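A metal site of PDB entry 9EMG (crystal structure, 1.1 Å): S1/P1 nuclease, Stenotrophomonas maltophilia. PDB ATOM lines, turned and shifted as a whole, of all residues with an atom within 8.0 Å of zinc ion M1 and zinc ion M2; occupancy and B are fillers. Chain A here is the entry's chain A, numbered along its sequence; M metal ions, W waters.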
ATOM      1  N   TRP A   1     -22.451  29.913  17.820  1.00  0.00           N
ATOM      2  CA  TRP A   1     -21.570  30.639  16.886  1.00  0.00           C
ATOM      3  C   TRP A   1     -20.271  29.867  16.701  1.00  0.00           C
ATOM      4  O   TRP A   1     -19.901  29.066  17.549  1.00  0.00           O
ATOM      5  CB  TRP A   1     -21.215  32.039  17.422  1.00  0.00           C
ATOM      6  CG  TRP A   1     -22.394  32.893  17.747  1.00  0.00           C
ATOM      7  CD1 TRP A   1     -22.953  33.074  18.969  1.00  0.00           C
ATOM      8  CD2 TRP A   1     -23.169  33.674  16.827  1.00  0.00           C
ATOM      9  NE1 TRP A   1     -24.000  33.925  18.887  1.00  0.00           N
ATOM     10  CE2 TRP A   1     -24.158  34.341  17.591  1.00  0.00           C
ATOM     11  CE3 TRP A   1     -23.095  33.947  15.451  1.00  0.00           C
ATOM     12  CZ2 TRP A   1     -25.101  35.173  17.014  1.00  0.00           C
ATOM     13  CZ3 TRP A   1     -24.012  34.807  14.890  1.00  0.00           C
ATOM     14  CH2 TRP A   1     -24.986  35.430  15.676  1.00  0.00           C
ATOM     15  N   GLY A   2     -19.570  30.188  15.629  1.00  0.00           N
ATOM     16  CA  GLY A   2     -18.153  29.860  15.526  1.00  0.00           C
ATOM     17  C   GLY A   2     -17.315  30.793  16.353  1.00  0.00           C
ATOM     18  O   GLY A   2     -17.829  31.641  17.125  1.00  0.00           O
ATOM     19  N   ALA A   3     -16.010  30.639  16.266  1.00  0.00           N
ATOM     20  CA  ALA A   3     -15.088  31.284  17.205  1.00  0.00           C
ATOM     21  C   ALA A   3     -15.166  32.806  17.112  1.00  0.00           C
ATOM     22  O   ALA A   3     -15.225  33.478  18.149  1.00  0.00           O
ATOM     23  CB  ALA A   3     -13.688  30.814  16.998  1.00  0.00           C
ATOM     24  N   GLY A   5     -17.700  34.767  16.197  1.00  0.00           N
ATOM     25  CA  GLY A   5     -18.915  35.288  16.835  1.00  0.00           C
ATOM     26  C   GLY A   5     -18.729  35.290  18.349  1.00  0.00           C
ATOM     27  O   GLY A   5     -19.123  36.231  19.035  1.00  0.00           O
ATOM     28  N   HIS A   6     -18.193  34.217  18.915  1.00  0.00           N
ATOM     29  CA  HIS A   6     -18.014  34.148  20.371  1.00  0.00           C
ATOM     30  C   HIS A   6     -17.073  35.253  20.858  1.00  0.00           C
ATOM     31  O   HIS A   6     -17.395  35.883  21.878  1.00  0.00           O
ATOM     32  CB  HIS A   6     -17.505  32.762  20.801  1.00  0.00           C
ATOM     33  CG  HIS A   6     -18.604  31.773  20.796  1.00  0.00           C
ATOM     34  ND1 HIS A   6     -19.629  31.874  21.715  1.00  0.00           N
ATOM     35  CD2 HIS A   6     -18.925  30.759  19.980  1.00  0.00           C
ATOM     36  CE1 HIS A   6     -20.553  30.936  21.414  1.00  0.00           C
ATOM     37  NE2 HIS A   6     -20.133  30.242  20.355  1.00  0.00           N
ATOM     38  N   ALA A  41     -13.577  33.039  25.027  1.00  0.00           N
ATOM     39  CA  ALA A  41     -14.959  32.922  24.539  1.00  0.00           C
ATOM     40  C   ALA A  41     -15.200  31.643  23.741  1.00  0.00           C
ATOM     41  O   ALA A  41     -16.293  31.056  23.890  1.00  0.00           O
ATOM     42  CB  ALA A  41     -15.395  34.161  23.829  1.00  0.00           C
ATOM     43  N   PRO A  42     -14.300  31.195  22.843  1.00  0.00           N
ATOM     44  CA  PRO A  42     -14.522  29.953  22.104  1.00  0.00           C
ATOM     45  C   PRO A  42     -14.240  28.670  22.874  1.00  0.00           C
ATOM     46  O   PRO A  42     -14.474  27.572  22.328  1.00  0.00           O
ATOM     47  CB  PRO A  42     -13.583  30.071  20.898  1.00  0.00           C
ATOM     48  CG  PRO A  42     -13.210  31.525  20.845  1.00  0.00           C
ATOM     49  CD  PRO A  42     -13.157  31.945  22.297  1.00  0.00           C
ATOM     50  N   TRP A  43     -13.668  28.775  24.076  1.00  0.00           N
ATOM     51  CA  TRP A  43     -13.098  27.616  24.811  1.00  0.00           C
ATOM     52  C   TRP A  43     -14.076  26.457  24.902  1.00  0.00           C
ATOM     53  O   TRP A  43     -13.689  25.300  24.642  1.00  0.00           O
ATOM     54  CB  TRP A  43     -12.609  28.079  26.177  1.00  0.00           C
ATOM     55  CG  TRP A  43     -12.157  27.007  27.124  1.00  0.00           C
ATOM     56  CD1 TRP A  43     -10.885  26.529  27.293  1.00  0.00           C
ATOM     57  CD2 TRP A  43     -12.959  26.335  28.104  1.00  0.00           C
ATOM     58  NE1 TRP A  43     -10.860  25.614  28.309  1.00  0.00           N
ATOM     59  CE2 TRP A  43     -12.119  25.479  28.829  1.00  0.00           C
ATOM     60  CE3 TRP A  43     -14.318  26.427  28.457  1.00  0.00           C
ATOM     61  CZ2 TRP A  43     -12.586  24.709  29.897  1.00  0.00           C
ATOM     62  CZ3 TRP A  43     -14.782  25.653  29.504  1.00  0.00           C
ATOM     63  CH2 TRP A  43     -13.932  24.812  30.203  1.00  0.00           C
ATOM     64  N   ALA A  44     -15.333  26.722  25.208  1.00  0.00           N
ATOM     65  CA  ALA A  44     -16.290  25.627  25.478  1.00  0.00           C
ATOM     66  C   ALA A  44     -16.506  24.785  24.219  1.00  0.00           C
ATOM     67  O   ALA A  44     -16.909  23.622  24.349  1.00  0.00           O
ATOM     68  CB  ALA A  44     -17.588  26.166  25.987  1.00  0.00           C
ATOM     69  N   ASP A  45     -16.318  25.341  23.027  1.00  0.00           N
ATOM     70  CA  ASP A  45     -16.422  24.558  21.773  1.00  0.00           C
ATOM     71  C   ASP A  45     -15.174  23.718  21.489  1.00  0.00           C
ATOM     72  O   ASP A  45     -15.225  22.877  20.586  1.00  0.00           O
ATOM     73  CB  ASP A  45     -16.685  25.477  20.589  1.00  0.00           C
ATOM     74  CG  ASP A  45     -18.106  25.950  20.412  1.00  0.00           C
ATOM     75  OD1 ASP A  45     -18.996  25.417  21.104  1.00  0.00           O
ATOM     76  OD2 ASP A  45     -18.313  26.854  19.583  1.00  0.00           O
ATOM     77  N   GLN A  46     -14.075  23.947  22.195  1.00  0.00           N
ATOM     78  CA  GLN A  46     -12.787  23.306  21.894  1.00  0.00           C
ATOM     79  C   GLN A  46     -12.537  22.098  22.809  1.00  0.00           C
ATOM     80  O   GLN A  46     -11.479  21.515  22.705  1.00  0.00           O
ATOM     81  CB  GLN A  46     -11.682  24.347  21.985  1.00  0.00           C
ATOM     82  CG  GLN A  46     -12.028  25.693  21.343  1.00  0.00           C
ATOM     83  CD  GLN A  46     -12.576  25.657  19.934  1.00  0.00           C
ATOM     84  OE1 GLN A  46     -12.156  24.848  19.106  1.00  0.00           O
ATOM     85  NE2 GLN A  46     -13.498  26.590  19.634  1.00  0.00           N
ATOM     86  N   SER A  58     -20.751  18.445  28.747  1.00  0.00           N
ATOM     87  CA  SER A  58     -21.263  19.787  28.415  1.00  0.00           C
ATOM     88  C   SER A  58     -21.718  19.964  26.952  1.00  0.00           C
ATOM     89  O   SER A  58     -22.149  21.040  26.588  1.00  0.00           O
ATOM     90  CB  SER A  58     -20.261  20.865  28.834  1.00  0.00           C
ATOM     91  OG  SER A  58     -19.086  20.765  28.055  1.00  0.00           O
ATOM     92  N   ALA A  59     -21.624  18.930  26.112  1.00  0.00           N
ATOM     93  CA  ALA A  59     -21.954  19.079  24.670  1.00  0.00           C
ATOM     94  C   ALA A  59     -23.363  19.636  24.503  1.00  0.00           C
ATOM     95  O   ALA A  59     -23.593  20.482  23.605  1.00  0.00           O
ATOM     96  CB  ALA A  59     -21.792  17.757  23.968  1.00  0.00           C
ATOM     97  N   TRP A  61     -25.097  21.492  26.369  1.00  0.00           N
ATOM     98  CA  TRP A  61     -25.325  22.795  27.010  1.00  0.00           C
ATOM     99  C   TRP A  61     -25.334  23.944  25.988  1.00  0.00           C
ATOM    100  O   TRP A  61     -25.635  25.059  26.382  1.00  0.00           O
ATOM    101  CB  TRP A  61     -24.250  23.079  28.044  1.00  0.00           C
ATOM    102  CG  TRP A  61     -24.177  22.139  29.194  1.00  0.00           C
ATOM    103  CD1 TRP A  61     -24.900  21.012  29.423  1.00  0.00           C
ATOM    104  CD2 TRP A  61     -23.211  22.247  30.252  1.00  0.00           C
ATOM    105  NE1 TRP A  61     -24.466  20.415  30.582  1.00  0.00           N
ATOM    106  CE2 TRP A  61     -23.439  21.152  31.117  1.00  0.00           C
ATOM    107  CE3 TRP A  61     -22.200  23.156  30.549  1.00  0.00           C
ATOM    108  CZ2 TRP A  61     -22.673  20.965  32.269  1.00  0.00           C
ATOM    109  CZ3 TRP A  61     -21.449  22.982  31.691  1.00  0.00           C
ATOM    110  CH2 TRP A  61     -21.679  21.886  32.519  1.00  0.00           C
ATOM    111  N   HIS A  62     -24.969  23.684  24.726  1.00  0.00           N
ATOM    112  CA  HIS A  62     -24.845  24.778  23.747  1.00  0.00           C
ATOM    113  C   HIS A  62     -26.177  25.097  23.067  1.00  0.00           C
ATOM    114  O   HIS A  62     -26.229  26.064  22.289  1.00  0.00           O
ATOM    115  CB  HIS A  62     -23.776  24.453  22.725  1.00  0.00           C
ATOM    116  CG  HIS A  62     -22.420  24.284  23.299  1.00  0.00           C
ATOM    117  ND1 HIS A  62     -21.339  25.036  22.892  1.00  0.00           N
ATOM    118  CD2 HIS A  62     -21.970  23.414  24.227  1.00  0.00           C
ATOM    119  CE1 HIS A  62     -20.269  24.615  23.565  1.00  0.00           C
ATOM    120  NE2 HIS A  62     -20.639  23.646  24.421  1.00  0.00           N
ATOM    121  N   TYR A  63     -27.231  24.297  23.294  1.00  0.00           N
ATOM    122  CA  TYR A  63     -28.492  24.334  22.505  1.00  0.00           C
ATOM    123  C   TYR A  63     -29.716  24.276  23.397  1.00  0.00           C
ATOM    124  O   TYR A  63     -29.663  23.728  24.518  1.00  0.00           O
ATOM    125  CB  TYR A  63     -28.602  23.151  21.529  1.00  0.00           C
ATOM    126  CG  TYR A  63     -27.305  22.758  20.878  1.00  0.00           C
ATOM    127  CD1 TYR A  63     -26.824  23.453  19.792  1.00  0.00           C
ATOM    128  CD2 TYR A  63     -26.514  21.753  21.389  1.00  0.00           C
ATOM    129  CE1 TYR A  63     -25.615  23.138  19.208  1.00  0.00           C
ATOM    130  CE2 TYR A  63     -25.305  21.420  20.832  1.00  0.00           C
ATOM    131  CZ  TYR A  63     -24.843  22.108  19.726  1.00  0.00           C
ATOM    132  OH  TYR A  63     -23.638  21.768  19.174  1.00  0.00           O
ATOM    133  N   ILE A  85     -29.006  24.690  27.158  1.00  0.00           N
ATOM    134  CA  ILE A  85     -28.343  25.987  27.418  1.00  0.00           C
ATOM    135  C   ILE A  85     -29.073  26.812  28.464  1.00  0.00           C
ATOM    136  O   ILE A  85     -28.392  27.576  29.158  1.00  0.00           O
ATOM    137  CB  ILE A  85     -28.171  26.764  26.103  1.00  0.00           C
ATOM    138  CG1 ILE A  85     -27.209  27.943  26.302  1.00  0.00           C
ATOM    139  CG2 ILE A  85     -29.482  27.189  25.466  1.00  0.00           C
ATOM    140  CD1 ILE A  85     -26.566  28.358  24.990  1.00  0.00           C
ATOM    141  N   HIS A 115     -19.339  32.017  26.877  1.00  0.00           N
ATOM    142  CA  HIS A 115     -19.671  31.243  25.654  1.00  0.00           C
ATOM    143  C   HIS A 115     -21.181  31.111  25.484  1.00  0.00           C
ATOM    144  O   HIS A 115     -21.716  31.309  24.412  1.00  0.00           O
ATOM    145  CB  HIS A 115     -19.028  29.862  25.723  1.00  0.00           C
ATOM    146  CG  HIS A 115     -19.183  29.085  24.464  1.00  0.00           C
ATOM    147  ND1 HIS A 115     -18.262  29.204  23.436  1.00  0.00           N
ATOM    148  CD2 HIS A 115     -20.150  28.260  24.024  1.00  0.00           C
ATOM    149  CE1 HIS A 115     -18.662  28.406  22.437  1.00  0.00           C
ATOM    150  NE2 HIS A 115     -19.814  27.836  22.777  1.00  0.00           N
ATOM    151  N   LEU A 116     -21.852  30.728  26.579  1.00  0.00           N
ATOM    152  CA  LEU A 116     -23.272  30.389  26.508  1.00  0.00           C
ATOM    153  C   LEU A 116     -24.125  31.637  26.303  1.00  0.00           C
ATOM    154  O   LEU A 116     -25.173  31.538  25.671  1.00  0.00           O
ATOM    155  CB  LEU A 116     -23.700  29.573  27.728  1.00  0.00           C
ATOM    156  CG  LEU A 116     -23.032  28.201  27.840  1.00  0.00           C
ATOM    157  CD1 LEU A 116     -23.516  27.482  29.099  1.00  0.00           C
ATOM    158  CD2 LEU A 116     -23.256  27.326  26.621  1.00  0.00           C
ATOM    159  N   GLY A 118     -23.296  33.914  24.386  1.00  0.00           N
ATOM    160  CA  GLY A 118     -23.210  33.976  22.922  1.00  0.00           C
ATOM    161  C   GLY A 118     -24.168  32.974  22.264  1.00  0.00           C
ATOM    162  O   GLY A 118     -25.001  33.322  21.432  1.00  0.00           O
ATOM    163  N   ASP A 119     -24.039  31.701  22.632  1.00  0.00           N
ATOM    164  CA  ASP A 119     -24.827  30.645  21.953  1.00  0.00           C
ATOM    165  C   ASP A 119     -26.328  30.844  22.120  1.00  0.00           C
ATOM    166  O   ASP A 119     -27.094  30.533  21.196  1.00  0.00           O
ATOM    167  CB  ASP A 119     -24.423  29.246  22.407  1.00  0.00           C
ATOM    168  CG  ASP A 119     -23.259  28.631  21.640  1.00  0.00           C
ATOM    169  OD1 ASP A 119     -22.900  29.238  20.611  1.00  0.00           O
ATOM    170  OD2 ASP A 119     -22.755  27.600  22.121  1.00  0.00           O
ATOM    171  N   ILE A 120     -26.793  31.367  23.263  1.00  0.00           N
ATOM    172  CA  ILE A 120     -28.243  31.469  23.508  1.00  0.00           C
ATOM    173  C   ILE A 120     -28.841  32.604  22.676  1.00  0.00           C
ATOM    174  O   ILE A 120     -30.078  32.690  22.613  1.00  0.00           O
ATOM    175  CB  ILE A 120     -28.526  31.581  25.026  1.00  0.00           C
ATOM    176  CG1 ILE A 120     -29.923  31.099  25.386  1.00  0.00           C
ATOM    177  CG2 ILE A 120     -28.259  32.985  25.534  1.00  0.00           C
ATOM    178  CD1 ILE A 120     -30.123  30.921  26.878  1.00  0.00           C
ATOM    179  N   GLN A 122     -27.762  32.838  19.403  1.00  0.00           N
ATOM    180  CA  GLN A 122     -27.664  32.302  18.029  1.00  0.00           C
ATOM    181  C   GLN A 122     -28.980  31.632  17.685  1.00  0.00           C
ATOM    182  O   GLN A 122     -29.310  30.609  18.290  1.00  0.00           O
ATOM    183  CB  GLN A 122     -26.491  31.343  17.980  1.00  0.00           C
ATOM    184  CG  GLN A 122     -26.477  30.494  16.726  1.00  0.00           C
ATOM    185  CD  GLN A 122     -26.627  31.281  15.442  1.00  0.00           C
ATOM    186  OE1 GLN A 122     -27.592  31.120  14.694  1.00  0.00           O
ATOM    187  NE2 GLN A 122     -25.682  32.151  15.172  1.00  0.00           N
ATOM    188  N   HIS A 125     -29.124  27.856  17.457  1.00  0.00           N
ATOM    189  CA  HIS A 125     -28.925  27.111  18.720  1.00  0.00           C
ATOM    190  C   HIS A 125     -30.215  27.027  19.543  1.00  0.00           C
ATOM    191  O   HIS A 125     -30.172  26.458  20.630  1.00  0.00           O
ATOM    192  CB  HIS A 125     -27.774  27.710  19.530  1.00  0.00           C
ATOM    193  CG  HIS A 125     -26.421  27.350  19.006  1.00  0.00           C
ATOM    194  ND1 HIS A 125     -25.443  26.822  19.815  1.00  0.00           N
ATOM    195  CD2 HIS A 125     -25.876  27.391  17.748  1.00  0.00           C
ATOM    196  CE1 HIS A 125     -24.383  26.532  19.071  1.00  0.00           C
ATOM    197  NE2 HIS A 125     -24.603  26.907  17.807  1.00  0.00           N
ATOM    198  N   HIS A 149     -27.264  25.798   9.721  1.00  0.00           N
ATOM    199  CA  HIS A 149     -26.641  26.021  11.034  1.00  0.00           C
ATOM    200  C   HIS A 149     -25.319  26.771  10.882  1.00  0.00           C
ATOM    201  O   HIS A 149     -25.109  27.817  11.521  1.00  0.00           O
ATOM    202  CB  HIS A 149     -26.523  24.702  11.782  1.00  0.00           C
ATOM    203  CG  HIS A 149     -26.075  24.904  13.189  1.00  0.00           C
ATOM    204  ND1 HIS A 149     -26.972  24.893  14.246  1.00  0.00           N
ATOM    205  CD2 HIS A 149     -24.855  25.195  13.718  1.00  0.00           C
ATOM    206  CE1 HIS A 149     -26.285  25.150  15.365  1.00  0.00           C
ATOM    207  NE2 HIS A 149     -25.003  25.338  15.097  1.00  0.00           N
ATOM    208  N   ASP A 153     -23.938  30.349  12.180  1.00  0.00           N
ATOM    209  CA  ASP A 153     -22.811  30.374  13.124  1.00  0.00           C
ATOM    210  C   ASP A 153     -21.644  31.225  12.600  1.00  0.00           C
ATOM    211  O   ASP A 153     -20.948  31.879  13.419  1.00  0.00           O
ATOM    212  CB  ASP A 153     -22.304  28.994  13.473  1.00  0.00           C
ATOM    213  CG  ASP A 153     -22.976  28.296  14.651  1.00  0.00           C
ATOM    214  OD1 ASP A 153     -23.836  28.881  15.301  1.00  0.00           O
ATOM    215  OD2 ASP A 153     -22.539  27.161  14.910  1.00  0.00           O
HETATM  216 ZN    ZN M   1     -20.996  26.578  21.596  1.00  0.00          ZN
HETATM  217 ZN    ZN M   2     -21.299  28.923  19.312  1.00  0.00          ZN
HETATM  218 ZN    ZN M   3     -23.558  26.152  16.246  1.00  0.00          ZN
HETATM  219  O   HOH W   1     -21.076  27.032  19.708  1.00  0.00           O
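Zinc ion M1 is bound by water W1 (1.9 Å), a ring nitrogen (ND1) of His 62 (2.0 Å), a ring nitrogen (NE2) of His 115 (2.1 Å), the side-chain carboxylate of Asp 119 (2.1 Å) and the side-chain carboxylate of Asp 45 (2.4 Å).
Of the 26 residues printed, 5 come within 4 Å of zinc ion M1.
Residues that only touch zinc ion M2: His 125 (3.9 Å).
Within 4 Å of zinc ion M2: Trp 1, His 6, Asp 45, His 115, Asp 119 and His 125.
The nearest printed residue that does not touch zinc ion M2 is Gly 2 (4.3 Å).
A ring nitrogen (ND1) of His 115 lies within hydrogen-bond range of the backbone carbonyl oxygen of Ala 41, 2.7 Å away.
The backbone carbonyl oxygen of Gly 118 is in hydrogen-bond range of the indole nitrogen of Trp 1 (2.8 Å).
The backbone NH of Trp 1 sits close to the side-chain carboxylate of Asp 153 (3.1 Å).
ND1 of His 6 lies close to O of His 115 (3.5 Å).
O of His 62 sits at hydrogen-bond distance from ND1 of His 125, at 2.7 Å.
Zinc ion M2 is bound by water W1, 1.9 Å away.
Zinc ion M2 is bound by NE2 of His 6.
Zinc ion M2 is bound by OD1 of Asp 119 (2.1 Å).
Zinc ion M2 is bound by N of Trp 1 (2.1 Å).
Zinc ion M2 is bound by O of Trp 1 (2.3 Å).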
